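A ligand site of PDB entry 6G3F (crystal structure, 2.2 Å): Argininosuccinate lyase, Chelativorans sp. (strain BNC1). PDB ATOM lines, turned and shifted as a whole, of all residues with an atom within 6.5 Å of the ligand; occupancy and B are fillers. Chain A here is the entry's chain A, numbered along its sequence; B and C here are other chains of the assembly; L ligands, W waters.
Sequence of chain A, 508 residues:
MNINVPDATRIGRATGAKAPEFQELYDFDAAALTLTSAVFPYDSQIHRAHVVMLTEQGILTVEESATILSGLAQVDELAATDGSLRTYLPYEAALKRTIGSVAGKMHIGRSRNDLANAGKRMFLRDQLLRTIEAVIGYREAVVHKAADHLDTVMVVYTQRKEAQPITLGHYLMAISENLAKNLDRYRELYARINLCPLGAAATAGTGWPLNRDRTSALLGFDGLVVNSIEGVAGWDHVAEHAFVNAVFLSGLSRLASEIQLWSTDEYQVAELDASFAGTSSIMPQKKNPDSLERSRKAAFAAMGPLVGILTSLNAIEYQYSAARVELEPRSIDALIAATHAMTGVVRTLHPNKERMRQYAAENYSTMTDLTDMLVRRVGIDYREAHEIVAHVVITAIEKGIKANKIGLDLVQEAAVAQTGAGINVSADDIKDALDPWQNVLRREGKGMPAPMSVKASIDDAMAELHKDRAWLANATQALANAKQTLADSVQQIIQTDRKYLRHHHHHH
The side-chain hydroxyl of Thr 158 of chain C lies within hydrogen-bond range of an oxygen (O3) of the ligand (2.9 Å). The side-chain hydroxyl (OG) of Ser 281 is in hydrogen-bond range of an oxygen (O2) of the ligand (2.7 Å). An oxygen (O1) of the ligand sits at hydrogen-bond distance from the backbone NH (N) of Ser 281. N of Arg 112 of chain B lies within hydrogen-bond range of O2 of the ligand (2.9 Å). The side-chain amino group (NZ) of Lys 286 lies within salt-bridge range of an oxygen (O4) of the ligand (2.5 Å). An oxygen (O1) of the ligand is in salt-bridge range of the guanidinium group (NE) of Arg 112 of chain B, at 2.8 Å. An oxygen (O3) of the ligand is in hydrogen-bond range of the side-chain amide nitrogen (ND2) of Asn 113 of chain B, at 2.8 Å. OG of Ser 111 of chain B lies within hydrogen-bond range of O2 of the ligand. An oxygen (O4) of the ligand lies close to the side-chain amide oxygen (OE1) of Gln 159 of chain C. An oxygen (O4) of the ligand sits at hydrogen-bond distance from the side-chain amide nitrogen (ND2) of Asn 288 (2.8 Å).
The side-chain hydroxyl (OG) of Ser 111 of chain B lies within hydrogen-bond range of the backbone NH (N) of Asn 113 of chain B. The side-chain amide nitrogen (ND2) of Asn 113 of chain B sits at hydrogen-bond distance from the backbone carbonyl oxygen (O) of Ala 202 of chain B (3.0 Å). The backbone carbonyl oxygen of Lys 286 is in hydrogen-bond range of the side-chain hydroxyl of Thr 279 (2.7 Å). The side-chain amino group (NZ) of Lys 286 is in hydrogen-bond range of the side-chain hydroxyl (OG1) of Thr 158 of chain C (2.7 Å). A ring nitrogen (NE2) of His 107 of chain B lies within hydrogen-bond range of the side-chain hydroxyl of Ser 281. The side-chain hydroxyl (OG) of Ser 280 is in hydrogen-bond range of the backbone NH (N) of Ile 282, 3.0 Å away. The backbone NH of Arg 112 of chain B sits at hydrogen-bond distance from the side-chain hydroxyl of Ser 281. OG of Ser 280 is in hydrogen-bond range of N of Met 283.
OG of Ser 280 touches C2 of the ligand, 2.9 Å away. Ile 282 touches the ligand. CE of Met 283 touches O4 of the ligand, 3.4 Å away. Tyr 320 of chain B touches the ligand. Hydrophobic or aromatic side chains that line the ligand: Ile 282, Met 283 and Tyr 320 of chain B. Of the 20 residues printed, 12 come within 4 Å of the ligand. The nearest printed residue that does not touch the ligand is Thr 279 (4.3 Å).
Water W2 lies within hydrogen-bond range of OD1 of Asn 113 of chain B (2.8 Å), O1 of the ligand (3.3 Å) and OH of Tyr 320 of chain B (3.3 Å).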
ATOM      1  N   THR A 279     -19.392  21.527  -7.379  1.00  0.00           N
ATOM      2  CA  THR A 279     -18.185  22.211  -7.799  1.00  0.00           C
ATOM      3  C   THR A 279     -17.696  23.096  -6.664  1.00  0.00           C
ATOM      4  O   THR A 279     -18.279  23.128  -5.565  1.00  0.00           O
ATOM      5  CB  THR A 279     -18.410  23.036  -9.078  1.00  0.00           C
ATOM      6  OG1 THR A 279     -17.142  23.463  -9.595  1.00  0.00           O
ATOM      7  CG2 THR A 279     -19.288  24.267  -8.793  1.00  0.00           C
ATOM      8  N   SER A 280     -16.607  23.817  -6.918  1.00  0.00           N
ATOM      9  CA  SER A 280     -15.948  24.637  -5.921  1.00  0.00           C
ATOM     10  C   SER A 280     -16.335  26.102  -6.087  1.00  0.00           C
ATOM     11  O   SER A 280     -16.601  26.577  -7.191  1.00  0.00           O
ATOM     12  CB  SER A 280     -14.441  24.496  -6.025  1.00  0.00           C
ATOM     13  OG  SER A 280     -13.770  25.443  -5.211  1.00  0.00           O
ATOM     14  N   SER A 281     -16.369  26.820  -4.957  1.00  0.00           N
ATOM     15  CA  SER A 281     -16.591  28.256  -4.999  1.00  0.00           C
ATOM     16  C   SER A 281     -15.368  29.026  -5.487  1.00  0.00           C
ATOM     17  O   SER A 281     -15.481  30.217  -5.768  1.00  0.00           O
ATOM     18  CB  SER A 281     -16.986  28.769  -3.602  1.00  0.00           C
ATOM     19  OG  SER A 281     -15.853  28.856  -2.750  1.00  0.00           O
ATOM     20  N   ILE A 282     -14.211  28.368  -5.599  1.00  0.00           N
ATOM     21  CA  ILE A 282     -12.961  29.040  -5.950  1.00  0.00           C
ATOM     22  C   ILE A 282     -12.308  28.390  -7.159  1.00  0.00           C
ATOM     23  O   ILE A 282     -11.727  29.072  -8.000  1.00  0.00           O
ATOM     24  CB  ILE A 282     -11.999  29.070  -4.750  1.00  0.00           C
ATOM     25  CG1 ILE A 282     -10.636  29.636  -5.170  1.00  0.00           C
ATOM     26  CG2 ILE A 282     -11.836  27.672  -4.165  1.00  0.00           C
ATOM     27  CD1 ILE A 282      -9.716  29.937  -4.003  1.00  0.00           C
ATOM     28  N   MET A 283     -12.388  27.061  -7.250  1.00  0.00           N
ATOM     29  CA  MET A 283     -11.689  26.311  -8.293  1.00  0.00           C
ATOM     30  C   MET A 283     -12.676  25.928  -9.399  1.00  0.00           C
ATOM     31  O   MET A 283     -13.470  24.994  -9.223  1.00  0.00           O
ATOM     32  CB  MET A 283     -11.032  25.064  -7.704  1.00  0.00           C
ATOM     33  CG  MET A 283      -9.844  25.370  -6.802  1.00  0.00           C
ATOM     34  SD  MET A 283      -9.195  23.965  -5.882  1.00  0.00           S
ATOM     35  CE  MET A 283     -10.577  23.583  -4.798  1.00  0.00           C
ATOM     36  N   LYS A 286     -13.308  22.097 -10.694  1.00  0.00           N
ATOM     37  CA  LYS A 286     -13.738  21.009  -9.818  1.00  0.00           C
ATOM     38  C   LYS A 286     -15.071  20.437 -10.262  1.00  0.00           C
ATOM     39  O   LYS A 286     -16.035  21.160 -10.498  1.00  0.00           O
ATOM     40  CB  LYS A 286     -13.841  21.489  -8.369  1.00  0.00           C
ATOM     41  CG  LYS A 286     -12.515  21.587  -7.626  1.00  0.00           C
ATOM     42  CD  LYS A 286     -11.745  20.265  -7.662  1.00  0.00           C
ATOM     43  CE  LYS A 286     -10.995  20.005  -6.377  1.00  0.00           C
ATOM     44  NZ  LYS A 286     -11.925  19.647  -5.269  1.00  0.00           N
ATOM     45  N   ASN A 288     -16.924  17.897  -8.062  1.00  0.00           N
ATOM     46  CA  ASN A 288     -16.638  17.288  -6.763  1.00  0.00           C
ATOM     47  C   ASN A 288     -17.628  16.175  -6.438  1.00  0.00           C
ATOM     48  O   ASN A 288     -18.826  16.306  -6.703  1.00  0.00           O
ATOM     49  CB  ASN A 288     -16.671  18.338  -5.664  1.00  0.00           C
ATOM     50  CG  ASN A 288     -15.419  19.199  -5.644  1.00  0.00           C
ATOM     51  OD1 ASN A 288     -14.334  18.745  -5.983  1.00  0.00           O
ATOM     52  ND2 ASN A 288     -15.580  20.448  -5.235  1.00  0.00           N
ATOM     53  N   LEU B  89     -22.787  29.944  -0.603  1.00  0.00           N
ATOM     54  CA  LEU B  89     -23.146  30.375  -1.953  1.00  0.00           C
ATOM     55  C   LEU B  89     -24.554  30.936  -2.046  1.00  0.00           C
ATOM     56  O   LEU B  89     -24.750  31.925  -2.764  1.00  0.00           O
ATOM     57  CB  LEU B  89     -22.941  29.211  -2.938  1.00  0.00           C
ATOM     58  CG  LEU B  89     -21.476  28.930  -3.292  1.00  0.00           C
ATOM     59  CD1 LEU B  89     -21.365  27.665  -4.122  1.00  0.00           C
ATOM     60  CD2 LEU B  89     -20.839  30.106  -4.046  1.00  0.00           C
ATOM     61  N   HIS B 107     -15.159  37.182  -1.850  1.00  0.00           N
ATOM     62  CA  HIS B 107     -14.579  35.848  -1.842  1.00  0.00           C
ATOM     63  C   HIS B 107     -13.172  35.815  -2.422  1.00  0.00           C
ATOM     64  O   HIS B 107     -12.606  34.733  -2.579  1.00  0.00           O
ATOM     65  CB  HIS B 107     -15.484  34.887  -2.617  1.00  0.00           C
ATOM     66  CG  HIS B 107     -15.436  33.482  -2.109  1.00  0.00           C
ATOM     67  ND1 HIS B 107     -15.510  33.169  -0.766  1.00  0.00           N
ATOM     68  CD2 HIS B 107     -15.336  32.296  -2.759  1.00  0.00           C
ATOM     69  CE1 HIS B 107     -15.448  31.860  -0.617  1.00  0.00           C
ATOM     70  NE2 HIS B 107     -15.343  31.303  -1.806  1.00  0.00           N
ATOM     71  N   ARG B 110     -10.203  33.468  -1.071  1.00  0.00           N
ATOM     72  CA  ARG B 110     -10.897  32.735  -0.031  1.00  0.00           C
ATOM     73  C   ARG B 110     -11.669  31.573  -0.643  1.00  0.00           C
ATOM     74  O   ARG B 110     -11.949  31.538  -1.843  1.00  0.00           O
ATOM     75  CB  ARG B 110     -11.851  33.659   0.733  1.00  0.00           C
ATOM     76  CG  ARG B 110     -12.390  33.096   2.027  1.00  0.00           C
ATOM     77  CD  ARG B 110     -13.278  34.103   2.731  1.00  0.00           C
ATOM     78  NE  ARG B 110     -14.473  34.397   1.950  1.00  0.00           N
ATOM     79  CZ  ARG B 110     -15.483  35.161   2.380  1.00  0.00           C
ATOM     80  NH1 ARG B 110     -15.433  35.706   3.583  1.00  0.00           N
ATOM     81  NH2 ARG B 110     -16.531  35.372   1.601  1.00  0.00           N
ATOM     82  N   SER B 111     -12.003  30.609   0.211  1.00  0.00           N
ATOM     83  CA  SER B 111     -12.746  29.428  -0.198  1.00  0.00           C
ATOM     84  C   SER B 111     -13.811  29.131   0.845  1.00  0.00           C
ATOM     85  O   SER B 111     -13.792  29.678   1.950  1.00  0.00           O
ATOM     86  CB  SER B 111     -11.805  28.218  -0.371  1.00  0.00           C
ATOM     87  OG  SER B 111     -12.532  27.005  -0.465  1.00  0.00           O
ATOM     88  N   ARG B 112     -14.748  28.249   0.499  1.00  0.00           N
ATOM     89  CA  ARG B 112     -15.628  27.698   1.514  1.00  0.00           C
ATOM     90  C   ARG B 112     -14.860  26.836   2.509  1.00  0.00           C
ATOM     91  O   ARG B 112     -15.318  26.654   3.637  1.00  0.00           O
ATOM     92  CB  ARG B 112     -16.755  26.891   0.869  1.00  0.00           C
ATOM     93  CG  ARG B 112     -17.795  27.747   0.147  1.00  0.00           C
ATOM     94  CD  ARG B 112     -18.964  26.916  -0.366  1.00  0.00           C
ATOM     95  NE  ARG B 112     -18.539  25.878  -1.304  1.00  0.00           N
ATOM     96  CZ  ARG B 112     -19.365  25.065  -1.943  1.00  0.00           C
ATOM     97  NH1 ARG B 112     -20.676  25.139  -1.752  1.00  0.00           N
ATOM     98  NH2 ARG B 112     -18.881  24.147  -2.767  1.00  0.00           N
ATOM     99  N   ASN B 113     -13.696  26.331   2.107  1.00  0.00           N
ATOM    100  CA  ASN B 113     -12.957  25.383   2.950  1.00  0.00           C
ATOM    101  C   ASN B 113     -12.367  26.074   4.173  1.00  0.00           C
ATOM    102  O   ASN B 113     -12.537  25.606   5.307  1.00  0.00           O
ATOM    103  CB  ASN B 113     -11.868  24.689   2.128  1.00  0.00           C
ATOM    104  CG  ASN B 113     -12.434  23.846   1.012  1.00  0.00           C
ATOM    105  OD1 ASN B 113     -13.642  23.607   0.941  1.00  0.00           O
ATOM    106  ND2 ASN B 113     -11.561  23.364   0.125  1.00  0.00           N
ATOM    107  N   ALA B 201      -7.336  29.489   1.931  1.00  0.00           N
ATOM    108  CA  ALA B 201      -8.240  29.416   0.779  1.00  0.00           C
ATOM    109  C   ALA B 201      -8.632  27.953   0.584  1.00  0.00           C
ATOM    110  O   ALA B 201      -9.079  27.311   1.546  1.00  0.00           O
ATOM    111  CB  ALA B 201      -7.590  30.077  -0.416  1.00  0.00           C
ATOM    112  N   ALA B 202      -8.486  27.379  -0.613  1.00  0.00           N
ATOM    113  CA  ALA B 202      -8.947  26.022  -0.852  1.00  0.00           C
ATOM    114  C   ALA B 202      -8.104  24.999  -0.098  1.00  0.00           C
ATOM    115  O   ALA B 202      -8.635  23.996   0.384  1.00  0.00           O
ATOM    116  CB  ALA B 202      -8.928  25.720  -2.352  1.00  0.00           C
ATOM    117  N   TYR B 320      -8.677  18.425   2.712  1.00  0.00           N
ATOM    118  CA  TYR B 320     -10.046  18.853   2.961  1.00  0.00           C
ATOM    119  C   TYR B 320     -10.976  17.770   2.440  1.00  0.00           C
ATOM    120  O   TYR B 320     -10.771  17.201   1.363  1.00  0.00           O
ATOM    121  CB  TYR B 320     -10.360  20.180   2.266  1.00  0.00           C
ATOM    122  CG  TYR B 320     -11.836  20.506   2.331  1.00  0.00           C
ATOM    123  CD1 TYR B 320     -12.366  21.154   3.435  1.00  0.00           C
ATOM    124  CD2 TYR B 320     -12.698  20.115   1.314  1.00  0.00           C
ATOM    125  CE1 TYR B 320     -13.716  21.438   3.510  1.00  0.00           C
ATOM    126  CE2 TYR B 320     -14.054  20.392   1.386  1.00  0.00           C
ATOM    127  CZ  TYR B 320     -14.555  21.056   2.493  1.00  0.00           C
ATOM    128  OH  TYR B 320     -15.897  21.334   2.570  1.00  0.00           O
ATOM    129  N   THR C 158      -8.182  18.049  -2.919  1.00  0.00           N
ATOM    130  CA  THR C 158      -9.306  18.203  -1.999  1.00  0.00           C
ATOM    131  C   THR C 158     -10.425  17.310  -2.501  1.00  0.00           C
ATOM    132  O   THR C 158     -10.727  17.309  -3.706  1.00  0.00           O
ATOM    133  CB  THR C 158      -9.790  19.653  -1.891  1.00  0.00           C
ATOM    134  OG1 THR C 158     -10.376  20.069  -3.125  1.00  0.00           O
ATOM    135  CG2 THR C 158      -8.640  20.584  -1.533  1.00  0.00           C
ATOM    136  N   GLN C 159     -11.036  16.555  -1.596  1.00  0.00           N
ATOM    137  CA  GLN C 159     -12.087  15.605  -1.972  1.00  0.00           C
ATOM    138  C   GLN C 159     -11.602  14.627  -3.030  1.00  0.00           C
ATOM    139  O   GLN C 159     -12.356  14.208  -3.912  1.00  0.00           O
ATOM    140  CB  GLN C 159     -13.340  16.346  -2.445  1.00  0.00           C
ATOM    141  CG  GLN C 159     -13.762  17.477  -1.505  1.00  0.00           C
ATOM    142  CD  GLN C 159     -15.095  18.087  -1.875  1.00  0.00           C
ATOM    143  OE1 GLN C 159     -15.163  19.177  -2.444  1.00  0.00           O
ATOM    144  NE2 GLN C 159     -16.183  17.392  -1.530  1.00  0.00           N
ATOM    145  N   LYS C 161      -9.787  15.134  -5.528  1.00  0.00           N
ATOM    146  CA  LYS C 161      -9.733  15.757  -6.847  1.00  0.00           C
ATOM    147  C   LYS C 161      -8.608  16.783  -6.864  1.00  0.00           C
ATOM    148  O   LYS C 161      -8.380  17.478  -5.864  1.00  0.00           O
ATOM    149  CB  LYS C 161     -11.072  16.442  -7.188  1.00  0.00           C
ATOM    150  CG  LYS C 161     -12.164  15.493  -7.677  1.00  0.00           C
ATOM    151  CD  LYS C 161     -11.749  14.806  -8.971  1.00  0.00           C
ATOM    152  CE  LYS C 161     -12.943  14.513  -9.863  1.00  0.00           C
ATOM    153  NZ  LYS C 161     -12.520  13.949 -11.169  1.00  0.00           N
ATOM    154  N   ALA C 163      -6.626  19.994  -7.036  1.00  0.00           N
ATOM    155  CA  ALA C 163      -7.080  21.311  -6.600  1.00  0.00           C
ATOM    156  C   ALA C 163      -6.183  22.414  -7.156  1.00  0.00           C
ATOM    157  O   ALA C 163      -6.596  23.142  -8.056  1.00  0.00           O
ATOM    158  CB  ALA C 163      -7.132  21.365  -5.070  1.00  0.00           C
HETATM  159  O1  LIG L   1     -16.071  25.362  -2.571  1.00  0.00           O
HETATM  160  C1  LIG L   1     -14.861  25.581  -2.308  1.00  0.00           C
HETATM  161  O2  LIG L   1     -14.495  26.715  -1.919  1.00  0.00           O
HETATM  162  C2  LIG L   1     -13.833  24.472  -2.498  1.00  0.00           C
HETATM  163  C3  LIG L   1     -14.228  23.265  -2.886  1.00  0.00           C
HETATM  164  C4  LIG L   1     -13.204  22.165  -3.087  1.00  0.00           C
HETATM  165  O3  LIG L   1     -12.359  21.903  -2.187  1.00  0.00           O
HETATM  166  O4  LIG L   1     -13.210  21.508  -4.159  1.00  0.00           O
HETATM  167  O   HOH W   1     -16.904  21.274  -1.864  1.00  0.00           O
HETATM  168  O   HOH W   2     -16.256  23.342  -0.002  1.00  0.00           O
